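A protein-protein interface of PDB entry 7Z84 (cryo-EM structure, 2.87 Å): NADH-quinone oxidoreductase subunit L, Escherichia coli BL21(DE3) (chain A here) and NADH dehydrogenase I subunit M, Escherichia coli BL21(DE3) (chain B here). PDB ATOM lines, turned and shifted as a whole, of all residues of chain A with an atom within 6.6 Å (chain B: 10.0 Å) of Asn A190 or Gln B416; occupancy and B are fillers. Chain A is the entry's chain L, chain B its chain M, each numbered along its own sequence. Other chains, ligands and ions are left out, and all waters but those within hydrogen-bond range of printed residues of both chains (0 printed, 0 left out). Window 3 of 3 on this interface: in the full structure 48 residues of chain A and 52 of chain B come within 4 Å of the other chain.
Leu A185 touches Phe B412 (O to CE1, 3.6 Å). Phe A186 touches Leu B411 (CZ to CB, 3.5 Å). Phe A186 touches Phe B415. CD2 of Phe A186 touches CG2 of Thr B422 (3.96 Å). CZ of Phe B415 touches CG1 of Ile A187 (3.6 Å). CE2 of Tyr A189 touches CD2 of Leu B336 (3.9 Å). CD2 of Tyr A189 touches CD1 of Phe B412, at 3.5 Å. Gln B416 touches Tyr A189 (OE1 to CE2, 3.8 Å). Phe B415 touches Asn A190. OD1 of Asn A190 touches NE2 of Gln B416, at 3.5 Å.
Hydrophobic or aromatic side chains of chain B within 4 Å of the printed part of chain A: Leu B336, Leu B411, Phe B412 and Phe B415. Among the printed residues, 11 pairs touch across the chains. Among the printed residues, no Asp or Glu carboxylate lies within 4 Å of a Lys or Arg side-chain nitrogen of the other chain.
Of the printed residues of chain B, Leu A185 touches Phe B412 (3.6 Å). Of the printed residues of chain B, Phe A186 touches Leu B411, Phe B412, Phe B415 and Thr B422. Printed residues of chain B within 4 Å of Tyr A189: Leu B336 (3.9 Å), Phe B412 (3.5 Å) and Gln B416 (3.8 Å). Of chain B, only Phe B415 and Gln B416 come within 4 Å of Asn A190. No residue of chain B comes within 4 Å of Glu A191. Gly B333 touches none of the printed residues of chain A. Printed residues of chain A within 4 Å of Phe B412: Leu A185 (3.6 Å), Phe A186 (3.5 Å) and Tyr A189 (3.5 Å). Of the printed residues of chain A, Phe B415 touches Phe A186 (3.7 Å), Ile A187 (3.6 Å) and Asn A190 (3.96 Å). Gln B416 touches two residues of chain A. Printed residues of chain A within 4 Å of Thr B422: Phe A186. The nearest residue of chain A that does not touch Gln B416 is Phe A186 (6.2 Å). The nearest printed residue of chain A that does not touch Thr B422 is Ile A187 (8.2 Å).
OG of Ser B334 lies close to N of Leu B336, 3.5 Å away. The backbone carbonyl oxygen (O) of Ser B414 lies close to the side-chain hydroxyl (OG1) of Thr B422 (3.5 Å). OG1 of Thr B422 lies within hydrogen-bond range of N of Phe B415. The side-chain hydroxyl (OG1) of Thr B422 lies within hydrogen-bond range of the backbone carbonyl oxygen (O) of Val B418.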
ATOM      1  N   LEU A 185       3.093  -4.849  -7.815  1.00  0.00           N
ATOM      2  CA  LEU A 185       2.014  -5.824  -7.964  1.00  0.00           C
ATOM      3  C   LEU A 185       2.511  -7.250  -7.745  1.00  0.00           C
ATOM      4  O   LEU A 185       1.844  -8.052  -7.076  1.00  0.00           O
ATOM      5  CB  LEU A 185       1.379  -5.697  -9.348  1.00  0.00           C
ATOM      6  CG  LEU A 185       0.058  -4.940  -9.485  1.00  0.00           C
ATOM      7  CD1 LEU A 185       0.258  -3.455  -9.280  1.00  0.00           C
ATOM      8  CD2 LEU A 185      -0.563  -5.209 -10.845  1.00  0.00           C
ATOM      9  N   PHE A 186       3.681  -7.580  -8.303  1.00  0.00           N
ATOM     10  CA  PHE A 186       4.228  -8.928  -8.160  1.00  0.00           C
ATOM     11  C   PHE A 186       4.567  -9.233  -6.709  1.00  0.00           C
ATOM     12  O   PHE A 186       4.247 -10.320  -6.210  1.00  0.00           O
ATOM     13  CB  PHE A 186       5.474  -9.112  -9.032  1.00  0.00           C
ATOM     14  CG  PHE A 186       5.248  -8.869 -10.498  1.00  0.00           C
ATOM     15  CD1 PHE A 186       4.006  -9.080 -11.075  1.00  0.00           C
ATOM     16  CD2 PHE A 186       6.286  -8.430 -11.300  1.00  0.00           C
ATOM     17  CE1 PHE A 186       3.803  -8.849 -12.416  1.00  0.00           C
ATOM     18  CE2 PHE A 186       6.088  -8.197 -12.643  1.00  0.00           C
ATOM     19  CZ  PHE A 186       4.843  -8.405 -13.200  1.00  0.00           C
ATOM     20  N   ILE A 187       5.198  -8.281  -6.013  1.00  0.00           N
ATOM     21  CA  ILE A 187       5.546  -8.490  -4.606  1.00  0.00           C
ATOM     22  C   ILE A 187       4.289  -8.638  -3.757  1.00  0.00           C
ATOM     23  O   ILE A 187       4.205  -9.524  -2.894  1.00  0.00           O
ATOM     24  CB  ILE A 187       6.444  -7.347  -4.097  1.00  0.00           C
ATOM     25  CG1 ILE A 187       7.774  -7.332  -4.847  1.00  0.00           C
ATOM     26  CG2 ILE A 187       6.706  -7.487  -2.607  1.00  0.00           C
ATOM     27  CD1 ILE A 187       8.486  -6.002  -4.794  1.00  0.00           C
ATOM     28  N   LEU A 188       3.281  -7.790  -4.002  1.00  0.00           N
ATOM     29  CA  LEU A 188       2.064  -7.837  -3.198  1.00  0.00           C
ATOM     30  C   LEU A 188       1.286  -9.129  -3.420  1.00  0.00           C
ATOM     31  O   LEU A 188       0.751  -9.701  -2.462  1.00  0.00           O
ATOM     32  CB  LEU A 188       1.193  -6.617  -3.493  1.00  0.00           C
ATOM     33  CG  LEU A 188       1.578  -5.383  -2.676  1.00  0.00           C
ATOM     34  CD1 LEU A 188       0.859  -4.144  -3.170  1.00  0.00           C
ATOM     35  CD2 LEU A 188       1.296  -5.618  -1.202  1.00  0.00           C
ATOM     36  N   TYR A 189       1.212  -9.615  -4.663  1.00  0.00           N
ATOM     37  CA  TYR A 189       0.527 -10.885  -4.893  1.00  0.00           C
ATOM     38  C   TYR A 189       1.328 -12.059  -4.343  1.00  0.00           C
ATOM     39  O   TYR A 189       0.746 -13.031  -3.849  1.00  0.00           O
ATOM     40  CB  TYR A 189       0.245 -11.092  -6.379  1.00  0.00           C
ATOM     41  CG  TYR A 189      -0.220 -12.498  -6.699  1.00  0.00           C
ATOM     42  CD1 TYR A 189      -1.481 -12.936  -6.313  1.00  0.00           C
ATOM     43  CD2 TYR A 189       0.611 -13.394  -7.361  1.00  0.00           C
ATOM     44  CE1 TYR A 189      -1.905 -14.221  -6.591  1.00  0.00           C
ATOM     45  CE2 TYR A 189       0.194 -14.680  -7.643  1.00  0.00           C
ATOM     46  CZ  TYR A 189      -1.063 -15.088  -7.255  1.00  0.00           C
ATOM     47  OH  TYR A 189      -1.480 -16.368  -7.534  1.00  0.00           O
ATOM     48  N   ASN A 190       2.660 -11.997  -4.425  1.00  0.00           N
ATOM     49  CA  ASN A 190       3.476 -13.085  -3.900  1.00  0.00           C
ATOM     50  C   ASN A 190       3.385 -13.177  -2.384  1.00  0.00           C
ATOM     51  O   ASN A 190       3.442 -14.279  -1.827  1.00  0.00           O
ATOM     52  CB  ASN A 190       4.930 -12.907  -4.332  1.00  0.00           C
ATOM     53  CG  ASN A 190       5.773 -14.132  -4.051  1.00  0.00           C
ATOM     54  OD1 ASN A 190       5.264 -15.251  -4.006  1.00  0.00           O
ATOM     55  ND2 ASN A 190       7.069 -13.926  -3.858  1.00  0.00           N
ATOM     56  N   GLU A 191       3.236 -12.043  -1.702  1.00  0.00           N
ATOM     57  CA  GLU A 191       3.170 -12.065  -0.246  1.00  0.00           C
ATOM     58  C   GLU A 191       1.757 -12.297   0.281  1.00  0.00           C
ATOM     59  O   GLU A 191       1.568 -13.073   1.222  1.00  0.00           O
ATOM     60  CB  GLU A 191       3.738 -10.764   0.322  1.00  0.00           C
ATOM     61  CG  GLU A 191       5.214 -10.565   0.038  1.00  0.00           C
ATOM     62  CD  GLU A 191       6.072 -11.656   0.642  1.00  0.00           C
ATOM     63  OE1 GLU A 191       5.802 -12.058   1.794  1.00  0.00           O
ATOM     64  OE2 GLU A 191       7.011 -12.121  -0.037  1.00  0.00           O
ATOM     65  N   LEU A 192       0.754 -11.637  -0.303  1.00  0.00           N
ATOM     66  CA  LEU A 192      -0.591 -11.666   0.255  1.00  0.00           C
ATOM     67  C   LEU A 192      -1.566 -12.540  -0.522  1.00  0.00           C
ATOM     68  O   LEU A 192      -2.588 -12.945   0.042  1.00  0.00           O
ATOM     69  CB  LEU A 192      -1.150 -10.242   0.346  1.00  0.00           C
ATOM     70  CG  LEU A 192      -0.292  -9.299   1.190  1.00  0.00           C
ATOM     71  CD1 LEU A 192      -0.838  -7.886   1.161  1.00  0.00           C
ATOM     72  CD2 LEU A 192      -0.196  -9.812   2.613  1.00  0.00           C
ATOM     73  N   GLY A 193      -1.287 -12.838  -1.787  1.00  0.00           N
ATOM     74  CA  GLY A 193      -2.171 -13.685  -2.561  1.00  0.00           C
ATOM     75  C   GLY A 193      -3.381 -12.994  -3.144  1.00  0.00           C
ATOM     76  O   GLY A 193      -4.225 -13.665  -3.749  1.00  0.00           O
ATOM     77  N   THR A 194      -3.497 -11.678  -2.986  1.00  0.00           N
ATOM     78  CA  THR A 194      -4.629 -10.938  -3.520  1.00  0.00           C
ATOM     79  C   THR A 194      -4.158  -9.563  -3.960  1.00  0.00           C
ATOM     80  O   THR A 194      -3.109  -9.076  -3.531  1.00  0.00           O
ATOM     81  CB  THR A 194      -5.759 -10.813  -2.491  1.00  0.00           C
ATOM     82  OG1 THR A 194      -6.848 -10.078  -3.061  1.00  0.00           O
ATOM     83  CG2 THR A 194      -5.267 -10.097  -1.245  1.00  0.00           C
ATOM     84  N   HIS A 207       0.236 -11.194   7.802  1.00  0.00           N
ATOM     85  CA  HIS A 207       1.328 -11.836   7.079  1.00  0.00           C
ATOM     86  C   HIS A 207       2.672 -11.183   7.382  1.00  0.00           C
ATOM     87  O   HIS A 207       3.694 -11.873   7.468  1.00  0.00           O
ATOM     88  CB  HIS A 207       1.050 -11.805   5.577  1.00  0.00           C
ATOM     89  CG  HIS A 207       2.159 -12.368   4.747  1.00  0.00           C
ATOM     90  ND1 HIS A 207       2.368 -13.723   4.603  1.00  0.00           N
ATOM     91  CD2 HIS A 207       3.126 -11.759   4.018  1.00  0.00           C
ATOM     92  CE1 HIS A 207       3.412 -13.925   3.820  1.00  0.00           C
ATOM     93  NE2 HIS A 207       3.891 -12.750   3.452  1.00  0.00           N
ATOM     94  N   MET A 214       9.555  -7.122   2.659  1.00  0.00           N
ATOM     95  CA  MET A 214       8.839  -7.282   1.397  1.00  0.00           C
ATOM     96  C   MET A 214       7.740  -6.237   1.240  1.00  0.00           C
ATOM     97  O   MET A 214       7.519  -5.725   0.137  1.00  0.00           O
ATOM     98  CB  MET A 214       8.263  -8.693   1.297  1.00  0.00           C
ATOM     99  CG  MET A 214       9.237  -9.842   0.931  1.00  0.00           C
ATOM    100  SD  MET A 214      10.220  -9.815  -0.603  1.00  0.00           S
ATOM    101  CE  MET A 214      11.616  -8.736  -0.263  1.00  0.00           C
ATOM    102  N   MET B 291      16.495 -20.214 -18.761  1.00  0.00           N
ATOM    103  CA  MET B 291      15.826 -18.948 -18.482  1.00  0.00           C
ATOM    104  C   MET B 291      16.751 -17.755 -18.696  1.00  0.00           C
ATOM    105  O   MET B 291      16.291 -16.682 -19.109  1.00  0.00           O
ATOM    106  CB  MET B 291      15.252 -18.966 -17.069  1.00  0.00           C
ATOM    107  CG  MET B 291      14.082 -19.922 -16.942  1.00  0.00           C
ATOM    108  SD  MET B 291      13.699 -20.358 -15.243  1.00  0.00           S
ATOM    109  CE  MET B 291      12.837 -18.880 -14.749  1.00  0.00           C
ATOM    110  N   THR B 332       9.799 -22.362 -15.364  1.00  0.00           N
ATOM    111  CA  THR B 332       9.493 -21.929 -14.006  1.00  0.00           C
ATOM    112  C   THR B 332       8.950 -23.063 -13.147  1.00  0.00           C
ATOM    113  O   THR B 332       9.279 -23.147 -11.959  1.00  0.00           O
ATOM    114  CB  THR B 332       8.478 -20.786 -14.025  1.00  0.00           C
ATOM    115  OG1 THR B 332       7.438 -21.091 -14.963  1.00  0.00           O
ATOM    116  CG2 THR B 332       9.143 -19.481 -14.416  1.00  0.00           C
ATOM    117  N   GLY B 333       8.131 -23.939 -13.722  1.00  0.00           N
ATOM    118  CA  GLY B 333       7.443 -24.941 -12.934  1.00  0.00           C
ATOM    119  C   GLY B 333       6.209 -24.428 -12.231  1.00  0.00           C
ATOM    120  O   GLY B 333       5.800 -25.002 -11.217  1.00  0.00           O
ATOM    121  N   SER B 334       5.599 -23.363 -12.745  1.00  0.00           N
ATOM    122  CA  SER B 334       4.447 -22.727 -12.123  1.00  0.00           C
ATOM    123  C   SER B 334       3.234 -22.839 -13.035  1.00  0.00           C
ATOM    124  O   SER B 334       3.341 -22.653 -14.251  1.00  0.00           O
ATOM    125  CB  SER B 334       4.735 -21.256 -11.811  1.00  0.00           C
ATOM    126  OG  SER B 334       3.589 -20.610 -11.285  1.00  0.00           O
ATOM    127  N   GLN B 335       2.083 -23.156 -12.436  1.00  0.00           N
ATOM    128  CA  GLN B 335       0.835 -23.256 -13.188  1.00  0.00           C
ATOM    129  C   GLN B 335       0.432 -21.909 -13.777  1.00  0.00           C
ATOM    130  O   GLN B 335      -0.008 -21.833 -14.933  1.00  0.00           O
ATOM    131  CB  GLN B 335      -0.268 -23.793 -12.277  1.00  0.00           C
ATOM    132  CG  GLN B 335      -1.663 -23.776 -12.875  1.00  0.00           C
ATOM    133  CD  GLN B 335      -2.148 -25.158 -13.252  1.00  0.00           C
ATOM    134  OE1 GLN B 335      -1.669 -26.159 -12.720  1.00  0.00           O
ATOM    135  NE2 GLN B 335      -3.112 -25.222 -14.161  1.00  0.00           N
ATOM    136  N   LEU B 336       0.579 -20.839 -12.990  1.00  0.00           N
ATOM    137  CA  LEU B 336       0.238 -19.497 -13.450  1.00  0.00           C
ATOM    138  C   LEU B 336       1.112 -19.075 -14.623  1.00  0.00           C
ATOM    139  O   LEU B 336       0.614 -18.533 -15.618  1.00  0.00           O
ATOM    140  CB  LEU B 336       0.384 -18.514 -12.288  1.00  0.00           C
ATOM    141  CG  LEU B 336      -0.099 -17.078 -12.469  1.00  0.00           C
ATOM    142  CD1 LEU B 336      -1.518 -17.077 -12.985  1.00  0.00           C
ATOM    143  CD2 LEU B 336      -0.001 -16.328 -11.156  1.00  0.00           C
ATOM    144  N   ALA B 337       2.416 -19.347 -14.533  1.00  0.00           N
ATOM    145  CA  ALA B 337       3.330 -19.000 -15.616  1.00  0.00           C
ATOM    146  C   ALA B 337       3.064 -19.835 -16.862  1.00  0.00           C
ATOM    147  O   ALA B 337       3.215 -19.345 -17.982  1.00  0.00           O
ATOM    148  CB  ALA B 337       4.776 -19.168 -15.154  1.00  0.00           C
ATOM    149  N   TYR B 338       2.645 -21.093 -16.689  1.00  0.00           N
ATOM    150  CA  TYR B 338       2.340 -21.936 -17.844  1.00  0.00           C
ATOM    151  C   TYR B 338       1.079 -21.462 -18.558  1.00  0.00           C
ATOM    152  O   TYR B 338       1.032 -21.425 -19.797  1.00  0.00           O
ATOM    153  CB  TYR B 338       2.170 -23.390 -17.410  1.00  0.00           C
ATOM    154  CG  TYR B 338       3.428 -24.130 -17.021  1.00  0.00           C
ATOM    155  CD1 TYR B 338       4.665 -23.507 -17.033  1.00  0.00           C
ATOM    156  CD2 TYR B 338       3.370 -25.462 -16.634  1.00  0.00           C
ATOM    157  CE1 TYR B 338       5.800 -24.182 -16.668  1.00  0.00           C
ATOM    158  CE2 TYR B 338       4.509 -26.150 -16.273  1.00  0.00           C
ATOM    159  CZ  TYR B 338       5.722 -25.505 -16.294  1.00  0.00           C
ATOM    160  OH  TYR B 338       6.863 -26.183 -15.936  1.00  0.00           O
ATOM    161  N   PHE B 408       1.884 -10.849 -18.298  1.00  0.00           N
ATOM    162  CA  PHE B 408       1.779 -10.563 -16.876  1.00  0.00           C
ATOM    163  C   PHE B 408       1.534 -11.823 -16.061  1.00  0.00           C
ATOM    164  O   PHE B 408       2.050 -11.937 -14.947  1.00  0.00           O
ATOM    165  CB  PHE B 408       0.703  -9.515 -16.617  1.00  0.00           C
ATOM    166  CG  PHE B 408       1.268  -8.168 -16.291  1.00  0.00           C
ATOM    167  CD1 PHE B 408       2.160  -7.556 -17.156  1.00  0.00           C
ATOM    168  CD2 PHE B 408       0.939  -7.530 -15.107  1.00  0.00           C
ATOM    169  CE1 PHE B 408       2.697  -6.323 -16.856  1.00  0.00           C
ATOM    170  CE2 PHE B 408       1.474  -6.295 -14.803  1.00  0.00           C
ATOM    171  CZ  PHE B 408       2.356  -5.695 -15.679  1.00  0.00           C
ATOM    172  N   MET B 409       0.782 -12.795 -16.591  1.00  0.00           N
ATOM    173  CA  MET B 409       0.684 -14.061 -15.867  1.00  0.00           C
ATOM    174  C   MET B 409       2.025 -14.791 -15.855  1.00  0.00           C
ATOM    175  O   MET B 409       2.388 -15.417 -14.846  1.00  0.00           O
ATOM    176  CB  MET B 409      -0.399 -14.954 -16.466  1.00  0.00           C
ATOM    177  CG  MET B 409      -1.771 -14.800 -15.846  1.00  0.00           C
ATOM    178  SD  MET B 409      -2.889 -16.089 -16.426  1.00  0.00           S
ATOM    179  CE  MET B 409      -3.174 -15.577 -18.111  1.00  0.00           C
ATOM    180  N   ILE B 410       2.777 -14.699 -16.961  1.00  0.00           N
ATOM    181  CA  ILE B 410       4.131 -15.251 -17.019  1.00  0.00           C
ATOM    182  C   ILE B 410       5.004 -14.635 -15.934  1.00  0.00           C
ATOM    183  O   ILE B 410       5.688 -15.341 -15.183  1.00  0.00           O
ATOM    184  CB  ILE B 410       4.741 -15.020 -18.415  1.00  0.00           C
ATOM    185  CG1 ILE B 410       4.174 -16.003 -19.431  1.00  0.00           C
ATOM    186  CG2 ILE B 410       6.262 -15.124 -18.378  1.00  0.00           C
ATOM    187  CD1 ILE B 410       4.595 -15.703 -20.850  1.00  0.00           C
ATOM    188  N   LEU B 411       4.972 -13.306 -15.823  1.00  0.00           N
ATOM    189  CA  LEU B 411       5.818 -12.618 -14.859  1.00  0.00           C
ATOM    190  C   LEU B 411       5.357 -12.857 -13.427  1.00  0.00           C
ATOM    191  O   LEU B 411       6.193 -12.922 -12.522  1.00  0.00           O
ATOM    192  CB  LEU B 411       5.853 -11.125 -15.170  1.00  0.00           C
ATOM    193  CG  LEU B 411       6.606 -10.723 -16.437  1.00  0.00           C
ATOM    194  CD1 LEU B 411       6.498  -9.231 -16.664  1.00  0.00           C
ATOM    195  CD2 LEU B 411       8.054 -11.161 -16.370  1.00  0.00           C
ATOM    196  N   PHE B 412       4.048 -13.003 -13.203  1.00  0.00           N
ATOM    197  CA  PHE B 412       3.546 -13.323 -11.870  1.00  0.00           C
ATOM    198  C   PHE B 412       4.044 -14.690 -11.413  1.00  0.00           C
ATOM    199  O   PHE B 412       4.565 -14.835 -10.299  1.00  0.00           O
ATOM    200  CB  PHE B 412       2.016 -13.280 -11.861  1.00  0.00           C
ATOM    201  CG  PHE B 412       1.440 -11.962 -11.414  1.00  0.00           C
ATOM    202  CD1 PHE B 412       1.603 -11.526 -10.113  1.00  0.00           C
ATOM    203  CD2 PHE B 412       0.709 -11.177 -12.287  1.00  0.00           C
ATOM    204  CE1 PHE B 412       1.067 -10.319  -9.703  1.00  0.00           C
ATOM    205  CE2 PHE B 412       0.173  -9.972 -11.884  1.00  0.00           C
ATOM    206  CZ  PHE B 412       0.350  -9.544 -10.588  1.00  0.00           C
ATOM    207  N   GLY B 413       3.916 -15.701 -12.279  1.00  0.00           N
ATOM    208  CA  GLY B 413       4.423 -17.023 -11.934  1.00  0.00           C
ATOM    209  C   GLY B 413       5.932 -17.053 -11.771  1.00  0.00           C
ATOM    210  O   GLY B 413       6.457 -17.693 -10.851  1.00  0.00           O
ATOM    211  N   SER B 414       6.651 -16.348 -12.650  1.00  0.00           N
ATOM    212  CA  SER B 414       8.106 -16.315 -12.569  1.00  0.00           C
ATOM    213  C   SER B 414       8.580 -15.619 -11.299  1.00  0.00           C
ATOM    214  O   SER B 414       9.535 -16.075 -10.662  1.00  0.00           O
ATOM    215  CB  SER B 414       8.683 -15.632 -13.807  1.00  0.00           C
ATOM    216  OG  SER B 414       9.912 -14.997 -13.510  1.00  0.00           O
ATOM    217  N   PHE B 415       7.925 -14.520 -10.908  1.00  0.00           N
ATOM    218  CA  PHE B 415       8.273 -13.852  -9.659  1.00  0.00           C
ATOM    219  C   PHE B 415       7.924 -14.712  -8.457  1.00  0.00           C
ATOM    220  O   PHE B 415       8.609 -14.642  -7.430  1.00  0.00           O
ATOM    221  CB  PHE B 415       7.570 -12.498  -9.564  1.00  0.00           C
ATOM    222  CG  PHE B 415       8.224 -11.548  -8.604  1.00  0.00           C
ATOM    223  CD1 PHE B 415       9.202 -10.673  -9.042  1.00  0.00           C
ATOM    224  CD2 PHE B 415       7.872 -11.535  -7.264  1.00  0.00           C
ATOM    225  CE1 PHE B 415       9.812  -9.799  -8.168  1.00  0.00           C
ATOM    226  CE2 PHE B 415       8.482 -10.666  -6.383  1.00  0.00           C
ATOM    227  CZ  PHE B 415       9.454  -9.797  -6.838  1.00  0.00           C
ATOM    228  N   GLN B 416       6.867 -15.522  -8.560  1.00  0.00           N
ATOM    229  CA  GLN B 416       6.630 -16.537  -7.539  1.00  0.00           C
ATOM    230  C   GLN B 416       7.751 -17.570  -7.514  1.00  0.00           C
ATOM    231  O   GLN B 416       7.997 -18.190  -6.474  1.00  0.00           O
ATOM    232  CB  GLN B 416       5.281 -17.215  -7.766  1.00  0.00           C
ATOM    233  CG  GLN B 416       4.090 -16.377  -7.338  1.00  0.00           C
ATOM    234  CD  GLN B 416       2.948 -17.216  -6.807  1.00  0.00           C
ATOM    235  OE1 GLN B 416       2.252 -17.891  -7.564  1.00  0.00           O
ATOM    236  NE2 GLN B 416       2.750 -17.181  -5.494  1.00  0.00           N
ATOM    237  N   VAL B 417       8.440 -17.769  -8.639  1.00  0.00           N
ATOM    238  CA  VAL B 417       9.581 -18.680  -8.673  1.00  0.00           C
ATOM    239  C   VAL B 417      10.890 -17.932  -8.420  1.00  0.00           C
ATOM    240  O   VAL B 417      11.575 -18.192  -7.425  1.00  0.00           O
ATOM    241  CB  VAL B 417       9.635 -19.447 -10.007  1.00  0.00           C
ATOM    242  CG1 VAL B 417      10.893 -20.295 -10.078  1.00  0.00           C
ATOM    243  CG2 VAL B 417       8.396 -20.319 -10.162  1.00  0.00           C
ATOM    244  N   VAL B 418      11.256 -17.006  -9.311  1.00  0.00           N
ATOM    245  CA  VAL B 418      12.529 -16.300  -9.238  1.00  0.00           C
ATOM    246  C   VAL B 418      12.348 -14.817  -9.546  1.00  0.00           C
ATOM    247  O   VAL B 418      11.821 -14.465 -10.605  1.00  0.00           O
ATOM    248  CB  VAL B 418      13.585 -16.913 -10.175  1.00  0.00           C
ATOM    249  CG1 VAL B 418      14.244 -18.118  -9.518  1.00  0.00           C
ATOM    250  CG2 VAL B 418      12.946 -17.339 -11.471  1.00  0.00           C
ATOM    251  N   PRO B 419      12.776 -13.910  -8.668  1.00  0.00           N
ATOM    252  CA  PRO B 419      12.479 -12.481  -8.864  1.00  0.00           C
ATOM    253  C   PRO B 419      13.353 -11.765  -9.889  1.00  0.00           C
ATOM    254  O   PRO B 419      12.873 -10.867 -10.595  1.00  0.00           O
ATOM    255  CB  PRO B 419      12.696 -11.889  -7.463  1.00  0.00           C
ATOM    256  CG  PRO B 419      12.760 -13.078  -6.525  1.00  0.00           C
ATOM    257  CD  PRO B 419      13.347 -14.173  -7.340  1.00  0.00           C
ATOM    258  N   VAL B 420      14.636 -12.134  -9.960  1.00  0.00           N
ATOM    259  CA  VAL B 420      15.605 -11.372 -10.749  1.00  0.00           C
ATOM    260  C   VAL B 420      15.307 -11.489 -12.239  1.00  0.00           C
ATOM    261  O   VAL B 420      15.330 -10.491 -12.975  1.00  0.00           O
ATOM    262  CB  VAL B 420      17.035 -11.837 -10.420  1.00  0.00           C
ATOM    263  CG1 VAL B 420      18.056 -10.945 -11.108  1.00  0.00           C
ATOM    264  CG2 VAL B 420      17.253 -11.849  -8.915  1.00  0.00           C
ATOM    265  N   ILE B 421      15.017 -12.706 -12.704  1.00  0.00           N
ATOM    266  CA  ILE B 421      14.665 -12.913 -14.104  1.00  0.00           C
ATOM    267  C   ILE B 421      13.376 -12.171 -14.438  1.00  0.00           C
ATOM    268  O   ILE B 421      13.236 -11.593 -15.523  1.00  0.00           O
ATOM    269  CB  ILE B 421      14.571 -14.423 -14.398  1.00  0.00           C
ATOM    270  CG1 ILE B 421      15.965 -15.050 -14.355  1.00  0.00           C
ATOM    271  CG2 ILE B 421      13.934 -14.697 -15.748  1.00  0.00           C
ATOM    272  CD1 ILE B 421      15.972 -16.504 -13.958  1.00  0.00           C
ATOM    273  N   THR B 422      12.447 -12.112 -13.479  1.00  0.00           N
ATOM    274  CA  THR B 422      11.191 -11.392 -13.674  1.00  0.00           C
ATOM    275  C   THR B 422      11.417  -9.891 -13.849  1.00  0.00           C
ATOM    276  O   THR B 422      10.830  -9.266 -14.745  1.00  0.00           O
ATOM    277  CB  THR B 422      10.260 -11.653 -12.491  1.00  0.00           C
ATOM    278  OG1 THR B 422      10.126 -13.063 -12.294  1.00  0.00           O
ATOM    279  CG2 THR B 422       8.895 -11.043 -12.741  1.00  0.00           C
ATOM    280  N   VAL B 423      12.260  -9.290 -13.004  1.00  0.00           N
ATOM    281  CA  VAL B 423      12.453  -7.843 -13.096  1.00  0.00           C
ATOM    282  C   VAL B 423      13.234  -7.480 -14.361  1.00  0.00           C
ATOM    283  O   VAL B 423      12.930  -6.477 -15.033  1.00  0.00           O
ATOM    284  CB  VAL B 423      13.092  -7.280 -11.805  1.00  0.00           C
ATOM    285  CG1 VAL B 423      12.233  -7.631 -10.597  1.00  0.00           C
ATOM    286  CG2 VAL B 423      14.519  -7.745 -11.583  1.00  0.00           C
ATOM    287  N   GLN B 497       2.431 -29.541 -15.090  1.00  0.00           N
ATOM    288  CA  GLN B 497       3.052 -28.929 -13.919  1.00  0.00           C
ATOM    289  C   GLN B 497       3.186 -29.920 -12.767  1.00  0.00           C
ATOM    290  O   GLN B 497       4.224 -29.954 -12.095  1.00  0.00           O
ATOM    291  CB  GLN B 497       2.246 -27.706 -13.484  1.00  0.00           C
ATOM    292  CG  GLN B 497       2.898 -26.890 -12.384  1.00  0.00           C
ATOM    293  CD  GLN B 497       2.312 -27.180 -11.017  1.00  0.00           C
ATOM    294  OE1 GLN B 497       1.166 -27.613 -10.901  1.00  0.00           O
ATOM    295  NE2 GLN B 497       3.097 -26.944  -9.974  1.00  0.00           N
